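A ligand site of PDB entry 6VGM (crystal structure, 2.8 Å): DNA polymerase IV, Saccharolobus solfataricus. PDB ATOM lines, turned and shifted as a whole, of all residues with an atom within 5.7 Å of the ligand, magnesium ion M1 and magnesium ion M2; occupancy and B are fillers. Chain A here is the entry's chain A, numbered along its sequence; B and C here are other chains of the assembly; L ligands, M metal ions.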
ATOM      1  N   ASP A   7      -0.993   4.913 -11.904  1.00  0.00           N
ATOM      2  CA  ASP A   7      -0.089   6.016 -11.642  1.00  0.00           C
ATOM      3  C   ASP A   7      -0.838   7.067 -10.844  1.00  0.00           C
ATOM      4  O   ASP A   7      -1.903   7.527 -11.265  1.00  0.00           O
ATOM      5  CB  ASP A   7       0.465   6.617 -12.937  1.00  0.00           C
ATOM      6  CG  ASP A   7       1.293   7.878 -12.689  1.00  0.00           C
ATOM      7  OD1 ASP A   7       0.697   8.958 -12.549  1.00  0.00           O
ATOM      8  OD2 ASP A   7       2.535   7.768 -12.612  1.00  0.00           O
ATOM      9  N   PHE A   8      -0.283   7.440  -9.697  1.00  0.00           N
ATOM     10  CA  PHE A   8      -0.952   8.361  -8.800  1.00  0.00           C
ATOM     11  C   PHE A   8      -1.007   9.757  -9.415  1.00  0.00           C
ATOM     12  O   PHE A   8      -0.163  10.132 -10.230  1.00  0.00           O
ATOM     13  CB  PHE A   8      -0.242   8.424  -7.444  1.00  0.00           C
ATOM     14  CG  PHE A   8       0.116   7.071  -6.881  1.00  0.00           C
ATOM     15  CD1 PHE A   8      -0.591   5.924  -7.239  1.00  0.00           C
ATOM     16  CD2 PHE A   8       1.165   6.947  -5.979  1.00  0.00           C
ATOM     17  CE1 PHE A   8      -0.251   4.687  -6.718  1.00  0.00           C
ATOM     18  CE2 PHE A   8       1.502   5.711  -5.449  1.00  0.00           C
ATOM     19  CZ  PHE A   8       0.797   4.578  -5.818  1.00  0.00           C
ATOM     20  N   ASP A   9      -2.033  10.522  -9.035  1.00  0.00           N
ATOM     21  CA  ASP A   9      -2.249  11.849  -9.588  1.00  0.00           C
ATOM     22  C   ASP A   9      -1.543  12.900  -8.747  1.00  0.00           C
ATOM     23  O   ASP A   9      -1.704  12.915  -7.517  1.00  0.00           O
ATOM     24  CB  ASP A   9      -3.747  12.155  -9.671  1.00  0.00           C
ATOM     25  CG  ASP A   9      -4.533  11.021 -10.293  1.00  0.00           C
ATOM     26  OD1 ASP A   9      -4.378  10.786 -11.516  1.00  0.00           O
ATOM     27  OD2 ASP A   9      -5.313  10.368  -9.570  1.00  0.00           O
ATOM     28  N   TYR A  10      -0.784  13.777  -9.403  1.00  0.00           N
ATOM     29  CA  TYR A  10       0.066  14.788  -8.762  1.00  0.00           C
ATOM     30  C   TYR A  10       0.594  14.292  -7.417  1.00  0.00           C
ATOM     31  O   TYR A  10       0.347  14.914  -6.384  1.00  0.00           O
ATOM     32  CB  TYR A  10      -0.683  16.127  -8.638  1.00  0.00           C
ATOM     33  CG  TYR A  10      -1.958  16.111  -7.804  1.00  0.00           C
ATOM     34  CD1 TYR A  10      -3.154  15.654  -8.329  1.00  0.00           C
ATOM     35  CD2 TYR A  10      -1.959  16.609  -6.504  1.00  0.00           C
ATOM     36  CE1 TYR A  10      -4.312  15.654  -7.570  1.00  0.00           C
ATOM     37  CE2 TYR A  10      -3.104  16.611  -5.741  1.00  0.00           C
ATOM     38  CZ  TYR A  10      -4.279  16.140  -6.279  1.00  0.00           C
ATOM     39  OH  TYR A  10      -5.425  16.155  -5.516  1.00  0.00           O
ATOM     40  N   PHE A  11       1.345  13.187  -7.435  1.00  0.00           N
ATOM     41  CA  PHE A  11       1.523  12.370  -6.235  1.00  0.00           C
ATOM     42  C   PHE A  11       2.042  13.170  -5.046  1.00  0.00           C
ATOM     43  O   PHE A  11       1.432  13.168  -3.969  1.00  0.00           O
ATOM     44  CB  PHE A  11       2.474  11.201  -6.539  1.00  0.00           C
ATOM     45  CG  PHE A  11       2.787  10.364  -5.332  1.00  0.00           C
ATOM     46  CD1 PHE A  11       1.762   9.833  -4.565  1.00  0.00           C
ATOM     47  CD2 PHE A  11       4.094  10.136  -4.949  1.00  0.00           C
ATOM     48  CE1 PHE A  11       2.048   9.066  -3.446  1.00  0.00           C
ATOM     49  CE2 PHE A  11       4.391   9.363  -3.836  1.00  0.00           C
ATOM     50  CZ  PHE A  11       3.369   8.832  -3.079  1.00  0.00           C
ATOM     51  N   TYR A  12       3.176  13.854  -5.215  1.00  0.00           N
ATOM     52  CA  TYR A  12       3.810  14.522  -4.084  1.00  0.00           C
ATOM     53  C   TYR A  12       2.877  15.537  -3.437  1.00  0.00           C
ATOM     54  O   TYR A  12       2.773  15.598  -2.209  1.00  0.00           O
ATOM     55  CB  TYR A  12       5.100  15.218  -4.538  1.00  0.00           C
ATOM     56  CG  TYR A  12       6.284  14.299  -4.713  1.00  0.00           C
ATOM     57  CD1 TYR A  12       6.130  12.918  -4.730  1.00  0.00           C
ATOM     58  CD2 TYR A  12       7.565  14.822  -4.874  1.00  0.00           C
ATOM     59  CE1 TYR A  12       7.222  12.087  -4.901  1.00  0.00           C
ATOM     60  CE2 TYR A  12       8.654  13.997  -5.057  1.00  0.00           C
ATOM     61  CZ  TYR A  12       8.478  12.630  -5.061  1.00  0.00           C
ATOM     62  OH  TYR A  12       9.563  11.805  -5.235  1.00  0.00           O
ATOM     63  N   ALA A  13       2.176  16.327  -4.251  1.00  0.00           N
ATOM     64  CA  ALA A  13       1.289  17.358  -3.716  1.00  0.00           C
ATOM     65  C   ALA A  13       0.096  16.751  -2.986  1.00  0.00           C
ATOM     66  O   ALA A  13      -0.286  17.224  -1.921  1.00  0.00           O
ATOM     67  CB  ALA A  13       0.820  18.277  -4.845  1.00  0.00           C
ATOM     68  N   VAL A  32      11.972  21.485  -4.874  1.00  0.00           N
ATOM     69  CA  VAL A  32      13.288  21.011  -4.477  1.00  0.00           C
ATOM     70  C   VAL A  32      14.179  22.242  -4.418  1.00  0.00           C
ATOM     71  O   VAL A  32      14.609  22.760  -5.455  1.00  0.00           O
ATOM     72  CB  VAL A  32      13.848  19.979  -5.463  1.00  0.00           C
ATOM     73  CG1 VAL A  32      15.020  19.212  -4.850  1.00  0.00           C
ATOM     74  CG2 VAL A  32      12.741  19.041  -5.934  1.00  0.00           C
ATOM     75  N   VAL A  43      10.702  22.545  -9.735  1.00  0.00           N
ATOM     76  CA  VAL A  43       9.386  22.118  -9.272  1.00  0.00           C
ATOM     77  C   VAL A  43       9.277  20.620  -9.491  1.00  0.00           C
ATOM     78  O   VAL A  43       9.383  20.139 -10.625  1.00  0.00           O
ATOM     79  CB  VAL A  43       8.258  22.889  -9.985  1.00  0.00           C
ATOM     80  CG1 VAL A  43       6.915  22.219  -9.723  1.00  0.00           C
ATOM     81  CG2 VAL A  43       8.231  24.330  -9.526  1.00  0.00           C
ATOM     82  N   ALA A  44       9.081  19.871  -8.399  1.00  0.00           N
ATOM     83  CA  ALA A  44       8.881  18.432  -8.505  1.00  0.00           C
ATOM     84  C   ALA A  44       7.536  18.122  -9.134  1.00  0.00           C
ATOM     85  O   ALA A  44       7.459  17.451 -10.177  1.00  0.00           O
ATOM     86  CB  ALA A  44       9.018  17.787  -7.127  1.00  0.00           C
ATOM     87  N   THR A  45       6.464  18.587  -8.514  1.00  0.00           N
ATOM     88  CA  THR A  45       5.136  18.474  -9.091  1.00  0.00           C
ATOM     89  C   THR A  45       4.261  19.585  -8.544  1.00  0.00           C
ATOM     90  O   THR A  45       4.578  20.212  -7.528  1.00  0.00           O
ATOM     91  CB  THR A  45       4.498  17.096  -8.817  1.00  0.00           C
ATOM     92  OG1 THR A  45       3.547  16.791  -9.845  1.00  0.00           O
ATOM     93  CG2 THR A  45       3.794  17.087  -7.455  1.00  0.00           C
ATOM     94  N   ALA A  46       3.164  19.854  -9.246  1.00  0.00           N
ATOM     95  CA  ALA A  46       2.150  20.787  -8.795  1.00  0.00           C
ATOM     96  C   ALA A  46       0.775  20.167  -9.038  1.00  0.00           C
ATOM     97  O   ALA A  46       0.578  19.430 -10.005  1.00  0.00           O
ATOM     98  CB  ALA A  46       2.249  22.136  -9.511  1.00  0.00           C
ATOM     99  N   TYR A  48      -3.323  20.054  -9.906  1.00  0.00           N
ATOM    100  CA  TYR A  48      -3.919  20.407 -11.195  1.00  0.00           C
ATOM    101  C   TYR A  48      -4.534  21.803 -11.205  1.00  0.00           C
ATOM    102  O   TYR A  48      -4.676  22.389 -12.285  1.00  0.00           O
ATOM    103  CB  TYR A  48      -4.946  19.359 -11.590  1.00  0.00           C
ATOM    104  CG  TYR A  48      -4.315  18.161 -12.255  1.00  0.00           C
ATOM    105  CD1 TYR A  48      -3.656  17.194 -11.491  1.00  0.00           C
ATOM    106  CD2 TYR A  48      -4.332  18.011 -13.629  1.00  0.00           C
ATOM    107  CE1 TYR A  48      -3.066  16.105 -12.090  1.00  0.00           C
ATOM    108  CE2 TYR A  48      -3.738  16.921 -14.238  1.00  0.00           C
ATOM    109  CZ  TYR A  48      -3.100  15.969 -13.461  1.00  0.00           C
ATOM    110  OH  TYR A  48      -2.510  14.879 -14.060  1.00  0.00           O
ATOM    111  N   ARG A  51      -1.354  23.382 -11.878  1.00  0.00           N
ATOM    112  CA  ARG A  51      -0.920  22.902 -13.190  1.00  0.00           C
ATOM    113  C   ARG A  51      -1.717  23.559 -14.311  1.00  0.00           C
ATOM    114  O   ARG A  51      -1.211  23.671 -15.442  1.00  0.00           O
ATOM    115  CB  ARG A  51      -1.041  21.377 -13.264  1.00  0.00           C
ATOM    116  CG  ARG A  51      -0.179  20.755 -14.349  1.00  0.00           C
ATOM    117  CD  ARG A  51      -0.244  19.226 -14.327  1.00  0.00           C
ATOM    118  NE  ARG A  51       0.108  18.674 -13.022  1.00  0.00           N
ATOM    119  CZ  ARG A  51       0.250  17.379 -12.775  1.00  0.00           C
ATOM    120  NH1 ARG A  51       0.076  16.494 -13.748  1.00  0.00           N
ATOM    121  NH2 ARG A  51       0.571  16.954 -11.562  1.00  0.00           N
ATOM    122  N   ALA A  57       6.221  20.026 -13.761  1.00  0.00           N
ATOM    123  CA  ALA A  57       7.477  19.439 -13.297  1.00  0.00           C
ATOM    124  C   ALA A  57       8.639  19.921 -14.160  1.00  0.00           C
ATOM    125  O   ALA A  57       8.525  20.024 -15.390  1.00  0.00           O
ATOM    126  CB  ALA A  57       7.385  17.918 -13.327  1.00  0.00           C
ATOM    127  N   GLY A  58       9.761  20.225 -13.517  1.00  0.00           N
ATOM    128  CA  GLY A  58      10.978  20.603 -14.196  1.00  0.00           C
ATOM    129  C   GLY A  58      11.201  22.082 -14.371  1.00  0.00           C
ATOM    130  O   GLY A  58      12.288  22.490 -14.801  1.00  0.00           O
ATOM    131  N   MET A  76      10.101  19.503  -0.494  1.00  0.00           N
ATOM    132  CA  MET A  76       9.790  18.094  -0.674  1.00  0.00           C
ATOM    133  C   MET A  76      10.164  17.291   0.564  1.00  0.00           C
ATOM    134  O   MET A  76      11.258  17.467   1.128  1.00  0.00           O
ATOM    135  CB  MET A  76      10.525  17.546  -1.905  1.00  0.00           C
ATOM    136  CG  MET A  76       9.906  16.305  -2.483  1.00  0.00           C
ATOM    137  SD  MET A  76      11.146  15.199  -3.184  1.00  0.00           S
ATOM    138  CE  MET A  76      12.311  16.355  -3.863  1.00  0.00           C
ATOM    139  N   SER A 103       8.090   3.109 -10.552  1.00  0.00           N
ATOM    140  CA  SER A 103       8.666   4.300  -9.946  1.00  0.00           C
ATOM    141  C   SER A 103       8.046   4.587  -8.576  1.00  0.00           C
ATOM    142  O   SER A 103       7.442   3.702  -7.970  1.00  0.00           O
ATOM    143  CB  SER A 103       8.473   5.527 -10.849  1.00  0.00           C
ATOM    144  OG  SER A 103       7.126   5.642 -11.283  1.00  0.00           O
ATOM    145  N   ILE A 104       8.206   5.821  -8.103  1.00  0.00           N
ATOM    146  CA  ILE A 104       7.637   6.206  -6.814  1.00  0.00           C
ATOM    147  C   ILE A 104       6.114   6.152  -6.848  1.00  0.00           C
ATOM    148  O   ILE A 104       5.473   5.925  -5.815  1.00  0.00           O
ATOM    149  CB  ILE A 104       8.144   7.606  -6.402  1.00  0.00           C
ATOM    150  CG1 ILE A 104       7.759   7.934  -4.959  1.00  0.00           C
ATOM    151  CG2 ILE A 104       7.597   8.682  -7.332  1.00  0.00           C
ATOM    152  CD1 ILE A 104       8.379   7.011  -3.934  1.00  0.00           C
ATOM    153  N   ASP A 105       5.501   6.333  -8.029  1.00  0.00           N
ATOM    154  CA  ASP A 105       4.050   6.472  -8.119  1.00  0.00           C
ATOM    155  C   ASP A 105       3.430   5.581  -9.193  1.00  0.00           C
ATOM    156  O   ASP A 105       2.283   5.811  -9.580  1.00  0.00           O
ATOM    157  CB  ASP A 105       3.670   7.945  -8.356  1.00  0.00           C
ATOM    158  CG  ASP A 105       3.703   8.345  -9.832  1.00  0.00           C
ATOM    159  OD1 ASP A 105       4.711   8.070 -10.527  1.00  0.00           O
ATOM    160  OD2 ASP A 105       2.727   8.957 -10.302  1.00  0.00           O
ATOM    161  N   GLU A 106       4.142   4.551  -9.643  1.00  0.00           N
ATOM    162  CA  GLU A 106       3.682   3.772 -10.790  1.00  0.00           C
ATOM    163  C   GLU A 106       3.823   2.278 -10.534  1.00  0.00           C
ATOM    164  O   GLU A 106       4.795   1.832  -9.924  1.00  0.00           O
ATOM    165  CB  GLU A 106       4.451   4.139 -12.059  1.00  0.00           C
ATOM    166  CG  GLU A 106       4.102   5.502 -12.588  1.00  0.00           C
ATOM    167  CD  GLU A 106       5.243   6.156 -13.329  1.00  0.00           C
ATOM    168  OE1 GLU A 106       5.466   5.786 -14.499  1.00  0.00           O
ATOM    169  OE2 GLU A 106       5.905   7.031 -12.741  1.00  0.00           O
ATOM    170  N   LYS A 159      -5.980  10.938 -16.811  1.00  0.00           N
ATOM    171  CA  LYS A 159      -5.638  11.740 -15.634  1.00  0.00           C
ATOM    172  C   LYS A 159      -6.447  13.040 -15.625  1.00  0.00           C
ATOM    173  O   LYS A 159      -6.557  13.695 -16.664  1.00  0.00           O
ATOM    174  CB  LYS A 159      -4.138  12.048 -15.598  1.00  0.00           C
ATOM    175  CG  LYS A 159      -3.254  10.863 -15.883  1.00  0.00           C
ATOM    176  CD  LYS A 159      -1.964  10.925 -15.083  1.00  0.00           C
ATOM    177  CE  LYS A 159      -2.210  10.609 -13.624  1.00  0.00           C
ATOM    178  NZ  LYS A 159      -1.828   9.242 -13.189  1.00  0.00           N
ATOM    179  N   PRO A 160      -6.991  13.466 -14.479  1.00  0.00           N
ATOM    180  CA  PRO A 160      -6.873  12.801 -13.170  1.00  0.00           C
ATOM    181  C   PRO A 160      -8.106  12.014 -12.745  1.00  0.00           C
ATOM    182  O   PRO A 160      -9.115  12.054 -13.447  1.00  0.00           O
ATOM    183  CB  PRO A 160      -6.646  13.979 -12.222  1.00  0.00           C
ATOM    184  CG  PRO A 160      -7.452  15.094 -12.843  1.00  0.00           C
ATOM    185  CD  PRO A 160      -7.573  14.810 -14.336  1.00  0.00           C
ATOM    186  P   A38 B   5      19.352  24.518  -8.836  1.00  0.00           P
ATOM    187  O1P A38 B   5      19.120  25.879  -8.331  1.00  0.00           O
ATOM    188  O2P A38 B   5      20.563  24.226  -9.648  1.00  0.00           O
ATOM    189  O5' A38 B   5      18.305  23.331  -8.518  1.00  0.00           O
ATOM    190  C5' A38 B   5      18.811  22.016  -8.477  1.00  0.00           C
ATOM    191  C4' A38 B   5      17.981  21.229  -7.478  1.00  0.00           C
ATOM    192  O4' A38 B   5      16.558  20.974  -8.073  1.00  0.00           O
ATOM    193  C3' A38 B   5      18.504  20.046  -7.288  1.00  0.00           C
ATOM    194  O3' A38 B   5      18.197  19.598  -5.941  1.00  0.00           O
ATOM    195  C2' A38 B   5      17.765  19.063  -8.347  1.00  0.00           C
ATOM    196  C1' A38 B   5      16.511  19.451  -8.290  1.00  0.00           C
ATOM    197  N9  A38 B   5      15.816  19.145  -9.566  1.00  0.00           N
ATOM    198  C8  A38 B   5      16.110  19.681 -10.857  1.00  0.00           C
ATOM    199  N7  A38 B   5      15.178  19.100 -11.791  1.00  0.00           N
ATOM    200  C5  A38 B   5      14.302  18.165 -11.048  1.00  0.00           C
ATOM    201  C6  A38 B   5      13.225  17.315 -11.394  1.00  0.00           C
ATOM    202  N6  A38 B   5      12.784  17.233 -12.757  1.00  0.00           N
ATOM    203  N1  A38 B   5      12.658  16.599 -10.430  1.00  0.00           N
ATOM    204  C2  A38 B   5      13.043  16.644  -9.151  1.00  0.00           C
ATOM    205  N3  A38 B   5      14.052  17.440  -8.794  1.00  0.00           N
ATOM    206  C4  A38 B   5      14.687  18.193  -9.703  1.00  0.00           C
ATOM    207  O   A38 B   5      16.947  20.469 -11.107  1.00  0.00           O
ATOM    208  P    DG B   6      19.621  19.297  -5.385  1.00  0.00           P
ATOM    209  OP1  DG B   6      19.420  19.664  -3.961  1.00  0.00           O
ATOM    210  OP2  DG B   6      20.916  19.560  -6.062  1.00  0.00           O
ATOM    211  O5'  DG B   6      19.248  17.757  -5.571  1.00  0.00           O
ATOM    212  C5'  DG B   6      18.087  17.229  -4.950  1.00  0.00           C
ATOM    213  C4'  DG B   6      17.648  15.938  -5.598  1.00  0.00           C
ATOM    214  O4'  DG B   6      17.136  16.179  -6.926  1.00  0.00           O
ATOM    215  C3'  DG B   6      18.741  14.871  -5.779  1.00  0.00           C
ATOM    216  O3'  DG B   6      18.478  13.793  -4.879  1.00  0.00           O
ATOM    217  C2'  DG B   6      18.607  14.424  -7.258  1.00  0.00           C
ATOM    218  C1'  DG B   6      17.217  14.960  -7.610  1.00  0.00           C
ATOM    219  N9   DG B   6      16.984  15.184  -9.038  1.00  0.00           N
ATOM    220  C8   DG B   6      17.658  16.044  -9.873  1.00  0.00           C
ATOM    221  N7   DG B   6      17.207  16.040 -11.104  1.00  0.00           N
ATOM    222  C5   DG B   6      16.169  15.118 -11.082  1.00  0.00           C
ATOM    223  C6   DG B   6      15.305  14.691 -12.115  1.00  0.00           C
ATOM    224  O6   DG B   6      15.288  15.058 -13.300  1.00  0.00           O
ATOM    225  N1   DG B   6      14.396  13.741 -11.671  1.00  0.00           N
ATOM    226  C2   DG B   6      14.315  13.268 -10.380  1.00  0.00           C
ATOM    227  N2   DG B   6      13.371  12.359 -10.142  1.00  0.00           N
ATOM    228  N3   DG B   6      15.117  13.667  -9.400  1.00  0.00           N
ATOM    229  C4   DG B   6      16.022  14.590  -9.823  1.00  0.00           C
ATOM    230  P    DC C  13       7.055   9.117 -17.133  1.00  0.00           P
ATOM    231  OP1  DC C  13       5.817   8.397 -17.523  1.00  0.00           O
ATOM    232  OP2  DC C  13       7.247  10.530 -17.519  1.00  0.00           O
ATOM    233  O5'  DC C  13       7.219   9.077 -15.536  1.00  0.00           O
ATOM    234  C5'  DC C  13       7.854   7.974 -14.882  1.00  0.00           C
ATOM    235  C4'  DC C  13       8.443   8.433 -13.556  1.00  0.00           C
ATOM    236  O4'  DC C  13       9.680   9.177 -13.775  1.00  0.00           O
ATOM    237  C3'  DC C  13       7.533   9.361 -12.747  1.00  0.00           C
ATOM    238  O3'  DC C  13       7.537   8.970 -11.375  1.00  0.00           O
ATOM    239  C2'  DC C  13       8.191  10.724 -12.929  1.00  0.00           C
ATOM    240  C1'  DC C  13       9.646  10.323 -12.953  1.00  0.00           C
ATOM    241  N1   DC C  13      10.539  11.392 -13.504  1.00  0.00           N
ATOM    242  C2   DC C  13      11.573  11.899 -12.711  1.00  0.00           C
ATOM    243  O2   DC C  13      11.747  11.432 -11.582  1.00  0.00           O
ATOM    244  N3   DC C  13      12.375  12.874 -13.216  1.00  0.00           N
ATOM    245  C4   DC C  13      12.157  13.347 -14.436  1.00  0.00           C
ATOM    246  N4   DC C  13      12.969  14.312 -14.885  1.00  0.00           N
ATOM    247  C5   DC C  13      11.103  12.851 -15.259  1.00  0.00           C
ATOM    248  C6   DC C  13      10.317  11.891 -14.759  1.00  0.00           C
HETATM  249  O1  LIG L   1      10.342  14.875  -8.901  1.00  0.00           O
HETATM  250  O2  LIG L   1      10.318  15.762 -13.351  1.00  0.00           O
HETATM  251  C1  LIG L   1       9.787  15.212 -12.381  1.00  0.00           C
HETATM  252  C2  LIG L   1       8.640  14.458 -12.513  1.00  0.00           C
HETATM  253  C3  LIG L   1       8.093  13.867 -11.386  1.00  0.00           C
HETATM  254  C4  LIG L   1       8.040  14.316 -13.760  1.00  0.00           C
HETATM  255  N1  LIG L   1      10.354  15.338 -11.123  1.00  0.00           N
HETATM  256  C5  LIG L   1       9.795  14.732 -10.001  1.00  0.00           C
HETATM  257  N2  LIG L   1       8.680  13.996 -10.100  1.00  0.00           N
HETATM  258  C6  LIG L   1       8.131  13.372  -8.835  1.00  0.00           C
HETATM  259  C7  LIG L   1       6.973  14.138  -8.195  1.00  0.00           C
HETATM  260  C8  LIG L   1       5.811  13.594  -9.003  1.00  0.00           C
HETATM  261  O3  LIG L   1       4.533  13.802  -8.318  1.00  0.00           O
HETATM  262  O4  LIG L   1       7.567  12.022  -8.854  1.00  0.00           O
HETATM  263  C9  LIG L   1       6.135  12.103  -9.085  1.00  0.00           C
HETATM  264  C10 LIG L   1       5.972  11.628 -10.520  1.00  0.00           C
HETATM  265  O5  LIG L   1       4.648  11.254 -10.861  1.00  0.00           O
HETATM  266  P1  LIG L   1       4.121  11.643 -12.308  1.00  0.00           P
HETATM  267  O6  LIG L   1       3.221  10.624 -12.913  1.00  0.00           O
HETATM  268  O7  LIG L   1       5.401  11.907 -13.257  1.00  0.00           O
HETATM  269  N3  LIG L   1       3.489  13.147 -12.169  1.00  0.00           N
HETATM  270  P2  LIG L   1       2.420  13.305 -10.926  1.00  0.00           P
HETATM  271  O8  LIG L   1       2.971  14.409  -9.898  1.00  0.00           O
HETATM  272  O9  LIG L   1       1.964  12.067 -10.228  1.00  0.00           O
HETATM  273  O10 LIG L   1       1.229  14.027 -11.661  1.00  0.00           O
HETATM  274  P3  LIG L   1       0.345  13.228 -12.717  1.00  0.00           P
HETATM  275  O11 LIG L   1       0.773  11.671 -12.716  1.00  0.00           O
HETATM  276  O12 LIG L   1      -1.098  13.401 -12.401  1.00  0.00           O
HETATM  277  O13 LIG L   1       0.757  13.766 -14.189  1.00  0.00           O
HETATM  278 MG    MG M   1       1.573  10.423 -11.195  1.00  0.00          MG
HETATM  279 MG    MG M   2       4.412   8.813 -13.270  1.00  0.00          MG
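DC 13 of chain C touches magnesium ion M2 (C3' to MG, 3.2 Å).
Magnesium ion M2 is bound by an oxygen (O6) of the ligand (2.2 Å), the side-chain carboxylate of Asp 7 (2.2 Å) and the side-chain carboxylate of Glu 106 (2.4 Å).
The side-chain hydroxyl of Thr 45 lies within hydrogen-bond range of an oxygen (O8) of the ligand (2.5 Å). O12 of the ligand is in hydrogen-bond range of OH of Tyr 48, at 2.6 Å. N1 of A38 5 of chain B is in hydrogen-bond range of a nitrogen (N1) of the ligand (2.7 Å). O13 of the ligand is in salt-bridge range of NH1 of Arg 51 (2.8 Å). An oxygen (O10) of the ligand lies within hydrogen-bond range of the backbone NH (N) of Tyr 10 (3.0 Å). N of Phe 11 is in hydrogen-bond range of O8 of the ligand (3.2 Å). The side-chain amino group (NZ) of Lys 159 sits close to an oxygen (O11) of the ligand. An oxygen (O3) of the ligand sits at hydrogen-bond distance from the backbone NH (N) of Tyr 12 (3.4 Å).
Magnesium ion M1 is bound by an oxygen (O9) of the ligand (1.9 Å), the backbone carbonyl oxygen (O) of Phe 8 (2.0 Å), the side-chain carboxylate (OD2) of Asp 105 (2.1 Å), an oxygen (O11) of the ligand (2.1 Å), the side-chain carboxylate (OD1) of Asp 7 (2.2 Å) and an oxygen (O6) of the ligand (2.4 Å). Magnesium ion M1 has six donor atoms within binding distance.
OE2 of Glu 106 lies close to OD1 of Asp 105, 2.7 Å away. NZ of Lys 159 sits at hydrogen-bond distance from O of Asp 7 (2.6 Å). OG1 of Thr 45 lies within hydrogen-bond range of NH2 of Arg 51 (3.4 Å). The guanidinium group (NH1) of Arg 51 sits at hydrogen-bond distance from the side-chain hydroxyl (OH) of Tyr 48, 3.1 Å away. The guanidinium group of Arg 51 lies within hydrogen-bond range of the backbone carbonyl oxygen of Ala 46, 2.9 Å away. N1 of DG 6 of chain B lies close to N3 of DC 13 of chain C (2.7 Å). The side-chain hydroxyl (OG) of Ser 103 lies within hydrogen-bond range of O3' of DC 13 of chain C, 3.4 Å away. The side-chain amino group (NZ) of Lys 159 lies within salt-bridge range of the side-chain carboxylate (OD1) of Asp 9 (3.4 Å).
O2 of the ligand lies close to N4 of DC 13 of chain C (3.4 Å). Asp 9 touches the ligand (CA to O12, 3.4 Å). Ala 44 touches the ligand. Ala 57 touches the ligand. CG2 of Ile 104 touches O4 of the ligand, at 3.7 Å. Hydrophobic or aromatic side chains that line the ligand: Phe 11, Tyr 12, Ala 44, Tyr 48, Ala 57 and Ile 104. Within 4 Å of the ligand: Asp 7, Phe 8, Asp 9, Tyr 10, Phe 11, Tyr 12, Ala 44, Thr 45, Tyr 48, Arg 51, Ala 57, Ile 104, Asp 105, Lys 159, A38 5 of chain B and DC 13 of chain C.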
